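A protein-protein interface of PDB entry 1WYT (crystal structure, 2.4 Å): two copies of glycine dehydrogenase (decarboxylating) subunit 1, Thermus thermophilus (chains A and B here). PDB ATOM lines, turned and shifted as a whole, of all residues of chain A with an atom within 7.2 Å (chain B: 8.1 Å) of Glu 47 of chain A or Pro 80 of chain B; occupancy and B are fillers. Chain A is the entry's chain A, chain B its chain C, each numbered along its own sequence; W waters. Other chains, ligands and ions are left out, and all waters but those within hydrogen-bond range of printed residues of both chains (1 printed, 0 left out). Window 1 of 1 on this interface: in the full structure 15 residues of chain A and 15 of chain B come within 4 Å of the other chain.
NE2 of His 77 of chain B lies within hydrogen-bond range of OE2 of Glu 47 of chain A (2.6 Å).
Hydrophobic or aromatic side chains of chain B within 4 Å of the printed part of chain A: His 77, Pro 79 and Pro 80. Hydrophobic or aromatic side chains of chain A that line the printed part of chain B: Trp 48. Along chain A the printed residues that touch a printed residue of chain B span positions 47 to 48. Among the printed residues, no Asp or Glu carboxylate lies within 4 Å of a Lys or Arg side-chain nitrogen of the other chain.
Water W1 lies within hydrogen-bond range of OE2 of Glu 47 of chain A and N of Val 81 of chain B.
Glu 47 of chain A touches just these residues of chain B: His 77, Pro 79 and Pro 80. Of chain A, only Glu 47 comes within 4 Å of Pro 80 of chain B. Of the printed residues of chain A, Pro 79 of chain B touches Glu 47. Printed residues of chain B within 4 Å of Trp 48 of chain A: His 77 (3.4 Å). Ala 86 of chain B touches none of the printed residues of chain A. The nearest residue of chain B that does not touch Glu 47 of chain A is Val 78 of chain B (5.3 Å). The nearest residue of chain A that does not touch Pro 80 of chain B is Leu 51 of chain A (4.5 Å). The nearest printed residue of chain B that does not touch Trp 48 of chain A is Val 78 of chain B (6.6 Å).
No position is printed for both chains. Of the 4 pairs that touch across the chains among the printed residues, none has its exchanged pair printed and touching as well.
Glu 47 of chain A touches Pro 79 of chain B (OE2 to CB, 3.8 Å). Pro 80 of chain B touches Glu 47 of chain A. Trp 48 of chain A touches His 77 of chain B (CB to ND1, 3.4 Å).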
ATOM      1  N   MET A   1     -11.243   3.946   5.284  1.00  0.00           N
ATOM      2  CA  MET A   1     -11.081   3.011   4.137  1.00  0.00           C
ATOM      3  C   MET A   1     -10.057   3.582   3.165  1.00  0.00           C
ATOM      4  O   MET A   1      -9.777   4.773   3.203  1.00  0.00           O
ATOM      5  CB  MET A   1     -12.420   2.822   3.431  1.00  0.00           C
ATOM      6  CG  MET A   1     -13.620   2.796   4.382  1.00  0.00           C
ATOM      7  SD  MET A   1     -13.396   1.833   5.912  1.00  0.00           S
ATOM      8  CE  MET A   1     -13.401   3.195   7.158  1.00  0.00           C
ATOM      9  N   TYR A   3      -7.815   3.051  -0.990  1.00  0.00           N
ATOM     10  CA  TYR A   3      -7.857   2.568  -2.364  1.00  0.00           C
ATOM     11  C   TYR A   3      -6.686   1.704  -2.813  1.00  0.00           C
ATOM     12  O   TYR A   3      -6.615   1.323  -3.982  1.00  0.00           O
ATOM     13  CB  TYR A   3      -7.986   3.770  -3.308  1.00  0.00           C
ATOM     14  CG  TYR A   3      -9.242   4.572  -3.061  1.00  0.00           C
ATOM     15  CD1 TYR A   3     -10.476   4.139  -3.548  1.00  0.00           C
ATOM     16  CD2 TYR A   3      -9.214   5.705  -2.252  1.00  0.00           C
ATOM     17  CE1 TYR A   3     -11.644   4.805  -3.230  1.00  0.00           C
ATOM     18  CE2 TYR A   3     -10.381   6.376  -1.928  1.00  0.00           C
ATOM     19  CZ  TYR A   3     -11.591   5.922  -2.418  1.00  0.00           C
ATOM     20  OH  TYR A   3     -12.749   6.589  -2.092  1.00  0.00           O
ATOM     21  N   LEU A  45     -13.970   7.037   7.441  1.00  0.00           N
ATOM     22  CA  LEU A  45     -15.357   6.620   7.288  1.00  0.00           C
ATOM     23  C   LEU A  45     -15.608   5.864   5.998  1.00  0.00           C
ATOM     24  O   LEU A  45     -14.951   6.105   4.981  1.00  0.00           O
ATOM     25  CB  LEU A  45     -16.283   7.830   7.287  1.00  0.00           C
ATOM     26  CG  LEU A  45     -16.379   8.738   8.504  1.00  0.00           C
ATOM     27  CD1 LEU A  45     -17.199   9.968   8.104  1.00  0.00           C
ATOM     28  CD2 LEU A  45     -17.020   8.002   9.671  1.00  0.00           C
ATOM     29  N   PRO A  46     -16.565   4.927   6.027  1.00  0.00           N
ATOM     30  CA  PRO A  46     -16.887   4.158   4.826  1.00  0.00           C
ATOM     31  C   PRO A  46     -17.534   5.125   3.836  1.00  0.00           C
ATOM     32  O   PRO A  46     -18.115   6.134   4.244  1.00  0.00           O
ATOM     33  CB  PRO A  46     -17.844   3.083   5.346  1.00  0.00           C
ATOM     34  CG  PRO A  46     -18.442   3.711   6.573  1.00  0.00           C
ATOM     35  CD  PRO A  46     -17.270   4.394   7.203  1.00  0.00           C
ATOM     36  N   GLU A  47     -17.423   4.836   2.544  1.00  0.00           N
ATOM     37  CA  GLU A  47     -17.975   5.738   1.550  1.00  0.00           C
ATOM     38  C   GLU A  47     -19.433   6.139   1.780  1.00  0.00           C
ATOM     39  O   GLU A  47     -19.763   7.321   1.659  1.00  0.00           O
ATOM     40  CB  GLU A  47     -17.781   5.174   0.135  1.00  0.00           C
ATOM     41  CG  GLU A  47     -18.571   3.929  -0.197  1.00  0.00           C
ATOM     42  CD  GLU A  47     -18.333   3.463  -1.630  1.00  0.00           C
ATOM     43  OE1 GLU A  47     -17.194   3.054  -1.953  1.00  0.00           O
ATOM     44  OE2 GLU A  47     -19.288   3.512  -2.433  1.00  0.00           O
ATOM     45  N   TRP A  48     -20.304   5.194   2.132  1.00  0.00           N
ATOM     46  CA  TRP A  48     -21.703   5.548   2.346  1.00  0.00           C
ATOM     47  C   TRP A  48     -21.863   6.584   3.456  1.00  0.00           C
ATOM     48  O   TRP A  48     -22.697   7.486   3.354  1.00  0.00           O
ATOM     49  CB  TRP A  48     -22.559   4.311   2.659  1.00  0.00           C
ATOM     50  CG  TRP A  48     -22.179   3.564   3.893  1.00  0.00           C
ATOM     51  CD1 TRP A  48     -21.336   2.497   3.975  1.00  0.00           C
ATOM     52  CD2 TRP A  48     -22.631   3.822   5.232  1.00  0.00           C
ATOM     53  NE1 TRP A  48     -21.234   2.073   5.276  1.00  0.00           N
ATOM     54  CE2 TRP A  48     -22.016   2.869   6.070  1.00  0.00           C
ATOM     55  CE3 TRP A  48     -23.493   4.771   5.805  1.00  0.00           C
ATOM     56  CZ2 TRP A  48     -22.234   2.833   7.454  1.00  0.00           C
ATOM     57  CZ3 TRP A  48     -23.711   4.735   7.181  1.00  0.00           C
ATOM     58  CH2 TRP A  48     -23.082   3.772   7.988  1.00  0.00           C
ATOM     59  N   LYS A  49     -21.060   6.465   4.508  1.00  0.00           N
ATOM     60  CA  LYS A  49     -21.129   7.406   5.620  1.00  0.00           C
ATOM     61  C   LYS A  49     -20.659   8.792   5.171  1.00  0.00           C
ATOM     62  O   LYS A  49     -21.177   9.805   5.635  1.00  0.00           O
ATOM     63  CB  LYS A  49     -20.276   6.908   6.790  1.00  0.00           C
ATOM     64  CG  LYS A  49     -20.340   7.788   8.019  1.00  0.00           C
ATOM     65  CD  LYS A  49     -21.590   7.530   8.835  1.00  0.00           C
ATOM     66  CE  LYS A  49     -21.426   6.295   9.726  1.00  0.00           C
ATOM     67  NZ  LYS A  49     -20.429   6.451  10.842  1.00  0.00           N
ATOM     68  N   VAL A  50     -19.682   8.833   4.266  1.00  0.00           N
ATOM     69  CA  VAL A  50     -19.169  10.101   3.740  1.00  0.00           C
ATOM     70  C   VAL A  50     -20.239  10.805   2.903  1.00  0.00           C
ATOM     71  O   VAL A  50     -20.336  12.030   2.903  1.00  0.00           O
ATOM     72  CB  VAL A  50     -17.902   9.880   2.864  1.00  0.00           C
ATOM     73  CG1 VAL A  50     -17.533  11.160   2.123  1.00  0.00           C
ATOM     74  CG2 VAL A  50     -16.748   9.444   3.738  1.00  0.00           C
ATOM     75  N   LEU A  51     -21.041  10.027   2.186  1.00  0.00           N
ATOM     76  CA  LEU A  51     -22.111  10.598   1.372  1.00  0.00           C
ATOM     77  C   LEU A  51     -23.223  11.152   2.259  1.00  0.00           C
ATOM     78  O   LEU A  51     -23.808  12.192   1.966  1.00  0.00           O
ATOM     79  CB  LEU A  51     -22.691   9.542   0.424  1.00  0.00           C
ATOM     80  CG  LEU A  51     -21.831   9.222  -0.795  1.00  0.00           C
ATOM     81  CD1 LEU A  51     -22.475   8.133  -1.618  1.00  0.00           C
ATOM     82  CD2 LEU A  51     -21.654  10.488  -1.618  1.00  0.00           C
ATOM     83  N   GLU A  52     -23.505  10.450   3.347  1.00  0.00           N
ATOM     84  CA  GLU A  52     -24.543  10.873   4.275  1.00  0.00           C
ATOM     85  C   GLU A  52     -24.161  12.226   4.861  1.00  0.00           C
ATOM     86  O   GLU A  52     -24.992  13.130   4.980  1.00  0.00           O
ATOM     87  CB  GLU A  52     -24.680   9.832   5.383  1.00  0.00           C
ATOM     88  CG  GLU A  52     -25.763  10.110   6.399  1.00  0.00           C
ATOM     89  CD  GLU A  52     -25.751   9.088   7.526  1.00  0.00           C
ATOM     90  OE1 GLU A  52     -25.840   7.873   7.225  1.00  0.00           O
ATOM     91  OE2 GLU A  52     -25.649   9.500   8.708  1.00  0.00           O
ATOM     92  N   GLU A  53     -22.889  12.355   5.221  1.00  0.00           N
ATOM     93  CA  GLU A  53     -22.373  13.587   5.791  1.00  0.00           C
ATOM     94  C   GLU A  53     -22.389  14.686   4.733  1.00  0.00           C
ATOM     95  O   GLU A  53     -22.698  15.841   5.028  1.00  0.00           O
ATOM     96  CB  GLU A  53     -20.955  13.357   6.318  1.00  0.00           C
ATOM     97  CG  GLU A  53     -20.340  14.542   7.048  1.00  0.00           C
ATOM     98  CD  GLU A  53     -21.280  15.182   8.057  1.00  0.00           C
ATOM     99  OE1 GLU A  53     -22.102  14.465   8.664  1.00  0.00           O
ATOM    100  OE2 GLU A  53     -21.184  16.410   8.252  1.00  0.00           O
ATOM    101  N   LEU A  54     -22.067  14.337   3.493  1.00  0.00           N
ATOM    102  CA  LEU A  54     -22.092  15.339   2.438  1.00  0.00           C
ATOM    103  C   LEU A  54     -23.524  15.815   2.209  1.00  0.00           C
ATOM    104  O   LEU A  54     -23.770  17.012   2.056  1.00  0.00           O
ATOM    105  CB  LEU A  54     -21.527  14.769   1.142  1.00  0.00           C
ATOM    106  CG  LEU A  54     -20.012  14.862   1.004  1.00  0.00           C
ATOM    107  CD1 LEU A  54     -19.550  13.957  -0.119  1.00  0.00           C
ATOM    108  CD2 LEU A  54     -19.604  16.312   0.750  1.00  0.00           C
ATOM    109  N   HIS B  77     -26.577   0.244   0.384  1.00  0.00           N
ATOM    110  CA  HIS B  77     -25.718   1.255  -0.219  1.00  0.00           C
ATOM    111  C   HIS B  77     -25.517   0.973  -1.703  1.00  0.00           C
ATOM    112  O   HIS B  77     -25.060  -0.110  -2.081  1.00  0.00           O
ATOM    113  CB  HIS B  77     -24.351   1.293   0.459  1.00  0.00           C
ATOM    114  CG  HIS B  77     -23.348   2.138  -0.268  1.00  0.00           C
ATOM    115  ND1 HIS B  77     -23.531   3.486  -0.487  1.00  0.00           N
ATOM    116  CD2 HIS B  77     -22.163   1.821  -0.840  1.00  0.00           C
ATOM    117  CE1 HIS B  77     -22.502   3.964  -1.162  1.00  0.00           C
ATOM    118  NE2 HIS B  77     -21.658   2.973  -1.389  1.00  0.00           N
ATOM    119  N   VAL B  78     -25.884   1.949  -2.531  1.00  0.00           N
ATOM    120  CA  VAL B  78     -25.739   1.872  -3.985  1.00  0.00           C
ATOM    121  C   VAL B  78     -24.384   2.520  -4.267  1.00  0.00           C
ATOM    122  O   VAL B  78     -24.249   3.742  -4.217  1.00  0.00           O
ATOM    123  CB  VAL B  78     -26.862   2.684  -4.699  1.00  0.00           C
ATOM    124  CG1 VAL B  78     -26.638   2.684  -6.216  1.00  0.00           C
ATOM    125  CG2 VAL B  78     -28.235   2.097  -4.351  1.00  0.00           C
ATOM    126  N   PRO B  79     -23.355   1.712  -4.554  1.00  0.00           N
ATOM    127  CA  PRO B  79     -22.040   2.300  -4.817  1.00  0.00           C
ATOM    128  C   PRO B  79     -21.907   3.069  -6.119  1.00  0.00           C
ATOM    129  O   PRO B  79     -22.173   2.543  -7.195  1.00  0.00           O
ATOM    130  CB  PRO B  79     -21.103   1.096  -4.735  1.00  0.00           C
ATOM    131  CG  PRO B  79     -21.963  -0.031  -5.169  1.00  0.00           C
ATOM    132  CD  PRO B  79     -23.269   0.243  -4.484  1.00  0.00           C
ATOM    133  N   PRO B  80     -21.490   4.340  -6.031  1.00  0.00           N
ATOM    134  CA  PRO B  80     -21.324   5.176  -7.219  1.00  0.00           C
ATOM    135  C   PRO B  80     -20.400   4.609  -8.289  1.00  0.00           C
ATOM    136  O   PRO B  80     -20.633   4.812  -9.483  1.00  0.00           O
ATOM    137  CB  PRO B  80     -20.829   6.509  -6.647  1.00  0.00           C
ATOM    138  CG  PRO B  80     -20.313   6.151  -5.269  1.00  0.00           C
ATOM    139  CD  PRO B  80     -21.296   5.132  -4.807  1.00  0.00           C
ATOM    140  N   VAL B  81     -19.361   3.886  -7.886  1.00  0.00           N
ATOM    141  CA  VAL B  81     -18.457   3.337  -8.886  1.00  0.00           C
ATOM    142  C   VAL B  81     -19.166   2.314  -9.775  1.00  0.00           C
ATOM    143  O   VAL B  81     -18.859   2.208 -10.960  1.00  0.00           O
ATOM    144  CB  VAL B  81     -17.203   2.689  -8.249  1.00  0.00           C
ATOM    145  CG1 VAL B  81     -17.586   1.487  -7.396  1.00  0.00           C
ATOM    146  CG2 VAL B  81     -16.248   2.277  -9.344  1.00  0.00           C
ATOM    147  N   VAL B  82     -20.114   1.572  -9.209  1.00  0.00           N
ATOM    148  CA  VAL B  82     -20.861   0.577  -9.977  1.00  0.00           C
ATOM    149  C   VAL B  82     -21.824   1.293 -10.913  1.00  0.00           C
ATOM    150  O   VAL B  82     -21.928   0.957 -12.097  1.00  0.00           O
ATOM    151  CB  VAL B  82     -21.675  -0.369  -9.056  1.00  0.00           C
ATOM    152  CG1 VAL B  82     -22.631  -1.227  -9.883  1.00  0.00           C
ATOM    153  CG2 VAL B  82     -20.729  -1.267  -8.270  1.00  0.00           C
ATOM    154  N   GLN B  83     -22.529   2.281 -10.371  1.00  0.00           N
ATOM    155  CA  GLN B  83     -23.479   3.051 -11.152  1.00  0.00           C
ATOM    156  C   GLN B  83     -22.765   3.839 -12.241  1.00  0.00           C
ATOM    157  O   GLN B  83     -23.287   3.996 -13.344  1.00  0.00           O
ATOM    158  CB  GLN B  83     -24.285   3.989 -10.239  1.00  0.00           C
ATOM    159  CG  GLN B  83     -25.325   3.250  -9.396  1.00  0.00           C
ATOM    160  CD  GLN B  83     -26.281   2.395 -10.245  1.00  0.00           C
ATOM    161  OE1 GLN B  83     -27.022   2.915 -11.086  1.00  0.00           O
ATOM    162  NE2 GLN B  83     -26.262   1.085 -10.024  1.00  0.00           N
ATOM    163  N   ALA B  84     -21.565   4.323 -11.944  1.00  0.00           N
ATOM    164  CA  ALA B  84     -20.805   5.081 -12.937  1.00  0.00           C
ATOM    165  C   ALA B  84     -20.386   4.160 -14.076  1.00  0.00           C
ATOM    166  O   ALA B  84     -20.427   4.546 -15.242  1.00  0.00           O
ATOM    167  CB  ALA B  84     -19.577   5.720 -12.297  1.00  0.00           C
ATOM    168  N   LEU B  85     -19.991   2.938 -13.738  1.00  0.00           N
ATOM    169  CA  LEU B  85     -19.566   1.963 -14.745  1.00  0.00           C
ATOM    170  C   LEU B  85     -20.721   1.460 -15.599  1.00  0.00           C
ATOM    171  O   LEU B  85     -20.587   1.338 -16.812  1.00  0.00           O
ATOM    172  CB  LEU B  85     -18.869   0.775 -14.078  1.00  0.00           C
ATOM    173  CG  LEU B  85     -17.533   1.146 -13.433  1.00  0.00           C
ATOM    174  CD1 LEU B  85     -17.005  -0.032 -12.629  1.00  0.00           C
ATOM    175  CD2 LEU B  85     -16.540   1.570 -14.531  1.00  0.00           C
ATOM    176  N   ALA B  86     -21.853   1.169 -14.967  1.00  0.00           N
ATOM    177  CA  ALA B  86     -23.019   0.689 -15.695  1.00  0.00           C
ATOM    178  C   ALA B  86     -23.630   1.797 -16.557  1.00  0.00           C
ATOM    179  O   ALA B  86     -24.504   1.533 -17.386  1.00  0.00           O
ATOM    180  CB  ALA B  86     -24.061   0.163 -14.719  1.00  0.00           C
ATOM    181  N   ALA B  87     -23.180   3.034 -16.351  1.00  0.00           N
ATOM    182  CA  ALA B  87     -23.702   4.172 -17.107  1.00  0.00           C
ATOM    183  C   ALA B  87     -22.955   4.385 -18.422  1.00  0.00           C
ATOM    184  O   ALA B  87     -23.388   5.158 -19.270  1.00  0.00           O
ATOM    185  CB  ALA B  87     -23.647   5.446 -16.257  1.00  0.00           C
ATOM    186  N   GLY B 259     -26.724  -4.025  -4.153  1.00  0.00           N
ATOM    187  CA  GLY B 259     -26.460  -2.629  -4.459  1.00  0.00           C
ATOM    188  C   GLY B 259     -27.361  -1.884  -5.427  1.00  0.00           C
ATOM    189  O   GLY B 259     -27.070  -0.737  -5.780  1.00  0.00           O
ATOM    190  N   TYR B 333     -21.060  -5.322  -8.659  1.00  0.00           N
ATOM    191  CA  TYR B 333     -21.155  -5.189  -7.213  1.00  0.00           C
ATOM    192  C   TYR B 333     -20.379  -6.310  -6.532  1.00  0.00           C
ATOM    193  O   TYR B 333     -19.528  -6.066  -5.679  1.00  0.00           O
ATOM    194  CB  TYR B 333     -22.627  -5.222  -6.794  1.00  0.00           C
ATOM    195  CG  TYR B 333     -22.859  -5.017  -5.316  1.00  0.00           C
ATOM    196  CD1 TYR B 333     -22.842  -3.738  -4.751  1.00  0.00           C
ATOM    197  CD2 TYR B 333     -23.114  -6.096  -4.485  1.00  0.00           C
ATOM    198  CE1 TYR B 333     -23.079  -3.547  -3.393  1.00  0.00           C
ATOM    199  CE2 TYR B 333     -23.350  -5.918  -3.131  1.00  0.00           C
ATOM    200  CZ  TYR B 333     -23.334  -4.645  -2.588  1.00  0.00           C
ATOM    201  OH  TYR B 333     -23.577  -4.489  -1.241  1.00  0.00           O
ATOM    202  N   ALA B 336     -16.891  -5.758  -7.054  1.00  0.00           N
ATOM    203  CA  ALA B 336     -16.404  -4.626  -6.275  1.00  0.00           C
ATOM    204  C   ALA B 336     -16.206  -4.978  -4.802  1.00  0.00           C
ATOM    205  O   ALA B 336     -15.290  -4.466  -4.161  1.00  0.00           O
ATOM    206  CB  ALA B 336     -17.361  -3.460  -6.403  1.00  0.00           C
ATOM    207  N   LEU B 337     -17.062  -5.848  -4.266  1.00  0.00           N
ATOM    208  CA  LEU B 337     -16.978  -6.238  -2.859  1.00  0.00           C
ATOM    209  C   LEU B 337     -16.142  -7.493  -2.607  1.00  0.00           C
ATOM    210  O   LEU B 337     -15.460  -7.603  -1.588  1.00  0.00           O
ATOM    211  CB  LEU B 337     -18.383  -6.454  -2.281  1.00  0.00           C
ATOM    212  CG  LEU B 337     -19.187  -5.287  -1.678  1.00  0.00           C
ATOM    213  CD1 LEU B 337     -18.394  -4.692  -0.528  1.00  0.00           C
ATOM    214  CD2 LEU B 337     -19.486  -4.213  -2.719  1.00  0.00           C
HETATM  215  O   HOH W   1     -18.148   3.732  -5.102  1.00  0.00           O
